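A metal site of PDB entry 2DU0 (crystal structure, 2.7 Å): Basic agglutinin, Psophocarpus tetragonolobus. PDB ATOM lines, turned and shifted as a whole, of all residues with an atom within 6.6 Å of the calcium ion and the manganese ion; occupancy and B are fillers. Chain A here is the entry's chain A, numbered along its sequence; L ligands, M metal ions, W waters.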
ATOM      1  N   ASP A  87      16.547   1.207  27.795  1.00  0.00           N
ATOM      2  CA  ASP A  87      17.492   1.693  26.794  1.00  0.00           C
ATOM      3  C   ASP A  87      18.848   0.987  26.878  1.00  0.00           C
ATOM      4  O   ASP A  87      19.617   0.962  25.906  1.00  0.00           O
ATOM      5  CB  ASP A  87      17.709   3.203  26.951  1.00  0.00           C
ATOM      6  CG  ASP A  87      16.653   4.014  26.253  1.00  0.00           C
ATOM      7  OD1 ASP A  87      15.589   4.262  26.848  1.00  0.00           O
ATOM      8  OD2 ASP A  87      16.889   4.383  25.080  1.00  0.00           O
ATOM      9  N   GLY A 104      16.697   7.861  29.341  1.00  0.00           N
ATOM     10  CA  GLY A 104      16.606   7.397  27.967  1.00  0.00           C
ATOM     11  C   GLY A 104      17.938   7.008  27.365  1.00  0.00           C
ATOM     12  O   GLY A 104      18.771   6.361  28.012  1.00  0.00           O
ATOM     13  N   GLY A 105      18.157   7.412  26.119  1.00  0.00           N
ATOM     14  CA  GLY A 105      19.391   7.083  25.435  1.00  0.00           C
ATOM     15  C   GLY A 105      20.654   7.648  26.050  1.00  0.00           C
ATOM     16  O   GLY A 105      21.751   7.351  25.572  1.00  0.00           O
ATOM     17  N   TYR A 106      20.508   8.468  27.081  1.00  0.00           N
ATOM     18  CA  TYR A 106      21.671   9.037  27.773  1.00  0.00           C
ATOM     19  C   TYR A 106      22.078   8.205  28.968  1.00  0.00           C
ATOM     20  O   TYR A 106      23.027   8.537  29.684  1.00  0.00           O
ATOM     21  CB  TYR A 106      21.371  10.468  28.173  1.00  0.00           C
ATOM     22  CG  TYR A 106      21.232  11.340  26.964  1.00  0.00           C
ATOM     23  CD1 TYR A 106      22.249  11.401  26.030  1.00  0.00           C
ATOM     24  CD2 TYR A 106      20.060  12.062  26.734  1.00  0.00           C
ATOM     25  CE1 TYR A 106      22.121  12.155  24.871  1.00  0.00           C
ATOM     26  CE2 TYR A 106      19.922  12.833  25.574  1.00  0.00           C
ATOM     27  CZ  TYR A 106      20.964  12.863  24.654  1.00  0.00           C
ATOM     28  OH  TYR A 106      20.828  13.589  23.489  1.00  0.00           O
ATOM     29  N   PHE A 107      21.353   7.111  29.186  1.00  0.00           N
ATOM     30  CA  PHE A 107      21.639   6.169  30.249  1.00  0.00           C
ATOM     31  C   PHE A 107      21.732   6.759  31.662  1.00  0.00           C
ATOM     32  O   PHE A 107      22.011   6.037  32.616  1.00  0.00           O
ATOM     33  CB  PHE A 107      22.938   5.438  29.927  1.00  0.00           C
ATOM     34  CG  PHE A 107      22.966   4.811  28.564  1.00  0.00           C
ATOM     35  CD1 PHE A 107      22.120   3.758  28.251  1.00  0.00           C
ATOM     36  CD2 PHE A 107      23.884   5.228  27.609  1.00  0.00           C
ATOM     37  CE1 PHE A 107      22.199   3.115  27.005  1.00  0.00           C
ATOM     38  CE2 PHE A 107      23.973   4.601  26.378  1.00  0.00           C
ATOM     39  CZ  PHE A 107      23.126   3.548  26.065  1.00  0.00           C
ATOM     40  N   GLU A 122      29.057   0.788  27.273  1.00  0.00           N
ATOM     41  CA  GLU A 122      27.607   0.630  27.215  1.00  0.00           C
ATOM     42  C   GLU A 122      27.122  -0.655  26.563  1.00  0.00           C
ATOM     43  O   GLU A 122      27.776  -1.248  25.703  1.00  0.00           O
ATOM     44  CB  GLU A 122      26.961   1.794  26.468  1.00  0.00           C
ATOM     45  CG  GLU A 122      27.307   1.798  24.995  1.00  0.00           C
ATOM     46  CD  GLU A 122      26.526   2.822  24.203  1.00  0.00           C
ATOM     47  OE1 GLU A 122      26.540   4.012  24.585  1.00  0.00           O
ATOM     48  OE2 GLU A 122      25.901   2.432  23.193  1.00  0.00           O
ATOM     49  N   ASP A 124      23.897  -1.108  24.874  1.00  0.00           N
ATOM     50  CA  ASP A 124      22.759  -0.406  24.305  1.00  0.00           C
ATOM     51  C   ASP A 124      21.749  -1.335  23.692  1.00  0.00           C
ATOM     52  O   ASP A 124      22.076  -2.170  22.845  1.00  0.00           O
ATOM     53  CB  ASP A 124      23.282   0.569  23.252  1.00  0.00           C
ATOM     54  CG  ASP A 124      22.340   1.742  23.031  1.00  0.00           C
ATOM     55  OD1 ASP A 124      21.111   1.568  23.179  1.00  0.00           O
ATOM     56  OD2 ASP A 124      22.841   2.840  22.700  1.00  0.00           O
ATOM     57  N   THR A 125      20.483  -1.162  24.095  1.00  0.00           N
ATOM     58  CA  THR A 125      19.430  -2.010  23.585  1.00  0.00           C
ATOM     59  C   THR A 125      18.381  -1.299  22.749  1.00  0.00           C
ATOM     60  O   THR A 125      17.512  -1.926  22.152  1.00  0.00           O
ATOM     61  CB  THR A 125      18.756  -2.748  24.743  1.00  0.00           C
ATOM     62  OG1 THR A 125      18.171  -1.789  25.629  1.00  0.00           O
ATOM     63  CG2 THR A 125      19.795  -3.579  25.486  1.00  0.00           C
ATOM     64  N   PHE A 126      18.464   0.035  22.710  1.00  0.00           N
ATOM     65  CA  PHE A 126      17.534   0.821  21.928  1.00  0.00           C
ATOM     66  C   PHE A 126      18.311   1.649  20.915  1.00  0.00           C
ATOM     67  O   PHE A 126      19.286   2.306  21.263  1.00  0.00           O
ATOM     68  CB  PHE A 126      16.718   1.737  22.828  1.00  0.00           C
ATOM     69  CG  PHE A 126      15.820   2.665  22.074  1.00  0.00           C
ATOM     70  CD1 PHE A 126      14.598   2.226  21.592  1.00  0.00           C
ATOM     71  CD2 PHE A 126      16.206   3.987  21.834  1.00  0.00           C
ATOM     72  CE1 PHE A 126      13.763   3.098  20.880  1.00  0.00           C
ATOM     73  CE2 PHE A 126      15.390   4.858  21.137  1.00  0.00           C
ATOM     74  CZ  PHE A 126      14.157   4.412  20.662  1.00  0.00           C
ATOM     75  N   ARG A 127      17.865   1.632  19.669  1.00  0.00           N
ATOM     76  CA  ARG A 127      18.559   2.382  18.643  1.00  0.00           C
ATOM     77  C   ARG A 127      18.119   3.833  18.495  1.00  0.00           C
ATOM     78  O   ARG A 127      17.065   4.127  17.937  1.00  0.00           O
ATOM     79  CB  ARG A 127      18.447   1.681  17.284  1.00  0.00           C
ATOM     80  CG  ARG A 127      19.372   2.303  16.232  1.00  0.00           C
ATOM     81  CD  ARG A 127      19.346   1.524  14.918  1.00  0.00           C
ATOM     82  NE  ARG A 127      20.366   2.018  13.991  1.00  0.00           N
ATOM     83  CZ  ARG A 127      20.530   1.567  12.752  1.00  0.00           C
ATOM     84  NH1 ARG A 127      19.737   0.608  12.278  1.00  0.00           N
ATOM     85  NH2 ARG A 127      21.501   2.048  11.987  1.00  0.00           N
ATOM     86  N   ASN A 128      18.949   4.744  19.004  1.00  0.00           N
ATOM     87  CA  ASN A 128      18.679   6.161  18.898  1.00  0.00           C
ATOM     88  C   ASN A 128      19.197   6.597  17.530  1.00  0.00           C
ATOM     89  O   ASN A 128      19.813   5.804  16.811  1.00  0.00           O
ATOM     90  CB  ASN A 128      19.369   6.928  20.029  1.00  0.00           C
ATOM     91  CG  ASN A 128      18.696   6.760  21.400  1.00  0.00           C
ATOM     92  OD1 ASN A 128      18.996   5.843  22.146  1.00  0.00           O
ATOM     93  ND2 ASN A 128      17.772   7.633  21.720  1.00  0.00           N
ATOM     94  N   TRP A 130      21.654   8.318  16.695  1.00  0.00           N
ATOM     95  CA  TRP A 130      23.110   8.240  16.619  1.00  0.00           C
ATOM     96  C   TRP A 130      23.652   6.820  16.800  1.00  0.00           C
ATOM     97  O   TRP A 130      24.862   6.624  16.828  1.00  0.00           O
ATOM     98  CB  TRP A 130      23.722   9.111  17.711  1.00  0.00           C
ATOM     99  CG  TRP A 130      23.338   8.632  19.068  1.00  0.00           C
ATOM    100  CD1 TRP A 130      23.733   7.470  19.682  1.00  0.00           C
ATOM    101  CD2 TRP A 130      22.408   9.250  19.970  1.00  0.00           C
ATOM    102  NE1 TRP A 130      23.122   7.332  20.896  1.00  0.00           N
ATOM    103  CE2 TRP A 130      22.296   8.414  21.093  1.00  0.00           C
ATOM    104  CE3 TRP A 130      21.668  10.442  19.923  1.00  0.00           C
ATOM    105  CZ2 TRP A 130      21.465   8.725  22.180  1.00  0.00           C
ATOM    106  CZ3 TRP A 130      20.842  10.744  21.010  1.00  0.00           C
ATOM    107  CH2 TRP A 130      20.754   9.898  22.118  1.00  0.00           C
ATOM    108  N   ASP A 131      22.760   5.840  16.913  1.00  0.00           N
ATOM    109  CA  ASP A 131      23.157   4.446  17.131  1.00  0.00           C
ATOM    110  C   ASP A 131      23.155   3.545  15.932  1.00  0.00           C
ATOM    111  O   ASP A 131      22.374   3.730  14.997  1.00  0.00           O
ATOM    112  CB  ASP A 131      22.208   3.731  18.121  1.00  0.00           C
ATOM    113  CG  ASP A 131      22.416   4.133  19.562  1.00  0.00           C
ATOM    114  OD1 ASP A 131      23.562   4.474  19.936  1.00  0.00           O
ATOM    115  OD2 ASP A 131      21.440   4.079  20.330  1.00  0.00           O
ATOM    116  N   PRO A 132      24.049   2.559  15.934  1.00  0.00           N
ATOM    117  CA  PRO A 132      24.098   1.596  14.825  1.00  0.00           C
ATOM    118  C   PRO A 132      23.071   0.549  15.258  1.00  0.00           C
ATOM    119  O   PRO A 132      22.314   0.794  16.200  1.00  0.00           O
ATOM    120  CB  PRO A 132      25.541   1.083  14.876  1.00  0.00           C
ATOM    121  CG  PRO A 132      25.900   1.225  16.313  1.00  0.00           C
ATOM    122  CD  PRO A 132      25.342   2.586  16.643  1.00  0.00           C
ATOM    123  N   GLN A 133      23.027  -0.604  14.601  1.00  0.00           N
ATOM    124  CA  GLN A 133      22.071  -1.626  14.994  1.00  0.00           C
ATOM    125  C   GLN A 133      22.246  -1.931  16.488  1.00  0.00           C
ATOM    126  O   GLN A 133      23.300  -1.681  17.065  1.00  0.00           O
ATOM    127  CB  GLN A 133      22.307  -2.916  14.187  1.00  0.00           C
ATOM    128  CG  GLN A 133      21.075  -3.476  13.476  1.00  0.00           C
ATOM    129  CD  GLN A 133      21.082  -3.245  11.950  1.00  0.00           C
ATOM    130  OE1 GLN A 133      21.043  -2.107  11.473  1.00  0.00           O
ATOM    131  NE2 GLN A 133      21.140  -4.346  11.191  1.00  0.00           N
ATOM    132  N   ILE A 134      21.204  -2.452  17.112  1.00  0.00           N
ATOM    133  CA  ILE A 134      21.287  -2.852  18.505  1.00  0.00           C
ATOM    134  C   ILE A 134      20.813  -4.291  18.600  1.00  0.00           C
ATOM    135  O   ILE A 134      20.140  -4.795  17.697  1.00  0.00           O
ATOM    136  CB  ILE A 134      20.437  -1.931  19.459  1.00  0.00           C
ATOM    137  CG1 ILE A 134      19.007  -1.757  18.938  1.00  0.00           C
ATOM    138  CG2 ILE A 134      21.122  -0.593  19.629  1.00  0.00           C
ATOM    139  CD1 ILE A 134      18.140  -2.984  19.088  1.00  0.00           C
ATOM    140  N   HIS A 136      24.190  -3.519  21.066  1.00  0.00           N
ATOM    141  CA  HIS A 136      25.588  -3.382  20.761  1.00  0.00           C
ATOM    142  C   HIS A 136      26.388  -2.908  21.957  1.00  0.00           C
ATOM    143  O   HIS A 136      25.855  -2.250  22.849  1.00  0.00           O
ATOM    144  CB  HIS A 136      25.803  -2.413  19.579  1.00  0.00           C
ATOM    145  CG  HIS A 136      25.298  -1.015  19.803  1.00  0.00           C
ATOM    146  ND1 HIS A 136      24.266  -0.474  19.075  1.00  0.00           N
ATOM    147  CD2 HIS A 136      25.741  -0.021  20.613  1.00  0.00           C
ATOM    148  CE1 HIS A 136      24.088   0.784  19.424  1.00  0.00           C
ATOM    149  NE2 HIS A 136      24.976   1.087  20.360  1.00  0.00           N
ATOM    150  N   GLY A 138      29.425  -0.624  23.252  1.00  0.00           N
ATOM    151  CA  GLY A 138      30.057   0.564  22.749  1.00  0.00           C
ATOM    152  C   GLY A 138      30.977   1.168  23.776  1.00  0.00           C
ATOM    153  O   GLY A 138      30.762   1.026  24.984  1.00  0.00           O
ATOM    154  N   ASP A 140      32.267   4.597  25.094  1.00  0.00           N
ATOM    155  CA  ASP A 140      31.927   6.002  25.072  1.00  0.00           C
ATOM    156  C   ASP A 140      32.917   6.865  25.839  1.00  0.00           C
ATOM    157  O   ASP A 140      33.351   6.499  26.926  1.00  0.00           O
ATOM    158  CB  ASP A 140      30.513   6.200  25.657  1.00  0.00           C
ATOM    159  CG  ASP A 140      29.463   5.284  25.003  1.00  0.00           C
ATOM    160  OD1 ASP A 140      29.619   4.931  23.806  1.00  0.00           O
ATOM    161  OD2 ASP A 140      28.482   4.932  25.666  1.00  0.00           O
ATOM    162  N   VAL A 144      27.640   9.819  24.231  1.00  0.00           N
ATOM    163  CA  VAL A 144      26.894   8.594  24.028  1.00  0.00           C
ATOM    164  C   VAL A 144      27.090   8.101  22.594  1.00  0.00           C
ATOM    165  O   VAL A 144      26.588   7.048  22.209  1.00  0.00           O
ATOM    166  CB  VAL A 144      25.384   8.840  24.342  1.00  0.00           C
ATOM    167  CG1 VAL A 144      24.508   7.811  23.668  1.00  0.00           C
ATOM    168  CG2 VAL A 144      25.153   8.795  25.852  1.00  0.00           C
ATOM    169  N   ILE A 145      27.828   8.877  21.804  1.00  0.00           N
ATOM    170  CA  ILE A 145      28.129   8.485  20.422  1.00  0.00           C
ATOM    171  C   ILE A 145      29.436   7.718  20.506  1.00  0.00           C
ATOM    172  O   ILE A 145      30.510   8.310  20.465  1.00  0.00           O
ATOM    173  CB  ILE A 145      28.368   9.685  19.498  1.00  0.00           C
ATOM    174  CG1 ILE A 145      27.109  10.545  19.409  1.00  0.00           C
ATOM    175  CG2 ILE A 145      28.739   9.194  18.102  1.00  0.00           C
ATOM    176  CD1 ILE A 145      27.275  11.740  18.495  1.00  0.00           C
ATOM    177  N   SER A 146      29.335   6.400  20.637  1.00  0.00           N
ATOM    178  CA  SER A 146      30.491   5.508  20.766  1.00  0.00           C
ATOM    179  C   SER A 146      31.640   5.696  19.771  1.00  0.00           C
ATOM    180  O   SER A 146      31.416   5.968  18.604  1.00  0.00           O
ATOM    181  CB  SER A 146      30.008   4.063  20.691  1.00  0.00           C
ATOM    182  OG  SER A 146      29.001   3.837  21.646  1.00  0.00           O
ATOM    183  N   THR A 149      32.109   0.310  18.284  1.00  0.00           N
ATOM    184  CA  THR A 149      30.885  -0.414  18.548  1.00  0.00           C
ATOM    185  C   THR A 149      30.960  -1.853  18.021  1.00  0.00           C
ATOM    186  O   THR A 149      31.648  -2.125  17.046  1.00  0.00           O
ATOM    187  CB  THR A 149      29.701   0.341  17.859  1.00  0.00           C
ATOM    188  OG1 THR A 149      29.196   1.353  18.743  1.00  0.00           O
ATOM    189  CG2 THR A 149      28.598  -0.589  17.449  1.00  0.00           C
HETATM  190  C1  LIG L   1      12.870   8.361  23.227  1.00  0.00           C
HETATM  191  C2  LIG L   1      14.258   8.247  23.911  1.00  0.00           C
HETATM  192  C3  LIG L   1      14.844   6.855  23.617  1.00  0.00           C
HETATM  193  C4  LIG L   1      13.870   5.781  24.144  1.00  0.00           C
HETATM  194  C5  LIG L   1      12.495   5.970  23.442  1.00  0.00           C
HETATM  195  C6  LIG L   1      11.514   4.915  23.960  1.00  0.00           C
HETATM  196  O1  LIG L   1      12.992   8.270  21.794  1.00  0.00           O
HETATM  197  O2  LIG L   1      15.140   9.262  23.434  1.00  0.00           O
HETATM  198  O3  LIG L   1      16.121   6.726  24.237  1.00  0.00           O
HETATM  199  O4  LIG L   1      13.709   5.930  25.564  1.00  0.00           O
HETATM  200  O5  LIG L   1      11.971   7.304  23.715  1.00  0.00           O
HETATM  201  O6  LIG L   1      10.236   5.066  23.311  1.00  0.00           O
HETATM  202 CA    CA M   1      20.699   3.944  22.555  1.00  0.00          CA
HETATM  203 MN    MN M   2      24.710   3.075  21.304  1.00  0.00          MN
HETATM  204  O   HOH W   1      22.043   5.731  23.344  1.00  0.00           O
HETATM  205  O   HOH W   2      26.751   3.850  20.457  1.00  0.00           O
HETATM  206  O   HOH W   3      24.780   5.068  22.740  1.00  0.00           O
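The side-chain amide nitrogen (ND2) of Asn 128 is in hydrogen-bond range of an oxygen (O3) of the ligand (3.1 Å).
The backbone NH (N) of Gly 105 lies within hydrogen-bond range of an oxygen (O3) of the ligand (2.9 Å).
O3 of the ligand is in hydrogen-bond range of OD2 of Asp 87, at 2.6 Å.
A ring nitrogen (ND1) of His 136 is in hydrogen-bond range of the backbone carbonyl oxygen (O) of Gln 133 (2.5 Å).
OD1 of Asp 131 sits close to NE1 of Trp 130 (3.0 Å).
The guanidinium group of Arg 127 is in hydrogen-bond range of the backbone carbonyl oxygen of Asp 131 (2.8 Å).
The side-chain carboxylate (OE1) of Glu 122 lies close to the side-chain carboxylate (OD2) of Asp 140.
N of Glu 122 is in hydrogen-bond range of O of Gly 138, 2.9 Å away.
Four residues have an atom within 4 Å of the calcium ion: Asp 124, Phe 126, Asn 128 and Asp 131.
The nearest printed residue that does not touch the calcium ion is Phe 107 (4.3 Å).
Within 4 Å of the manganese ion: Glu 122, Asp 124, Asp 131 and His 136.
Along chain A the residues within 4 Å of the manganese ion span positions 122 to 136.
The nearest printed residue that does not touch the manganese ion is Ser 146 (4.4 Å).
The calcium ion is bound by the side-chain carboxylate (OD2) of Asp 131.
Water W1 is bound to the calcium ion (2.4 Å).
The side-chain carboxylate (OD2) of Asp 124 binds the calcium ion (2.4 Å).
The calcium ion is bound by the side-chain carboxylate (OD1) of Asp 124 (2.5 Å).
O of Phe 126 is bound to the calcium ion, 2.5 Å away.
The calcium ion is bound by the side-chain amide oxygen (OD1) of Asn 128 (2.6 Å).
The manganese ion is bound by NE2 of His 136 (2.2 Å).
The manganese ion is bound by OD1 of Asp 131 (2.3 Å).
The manganese ion is bound by the side-chain carboxylate (OE2) of Glu 122 (2.3 Å).
The manganese ion is bound by water W2 (2.3 Å).
The side-chain carboxylate (OD2) of Asp 124 is bound to the manganese ion.
Water W3 binds the manganese ion (2.5 Å).
Water W1 bridges O of Gly 105 (2.8 Å) and NE1 of Trp 130 (3.1 Å).
Water W3 lies within hydrogen-bond range of O of Val 144 (2.7 Å), OE1 of Glu 122 (2.8 Å) and NE1 of Trp 130 (3.4 Å).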
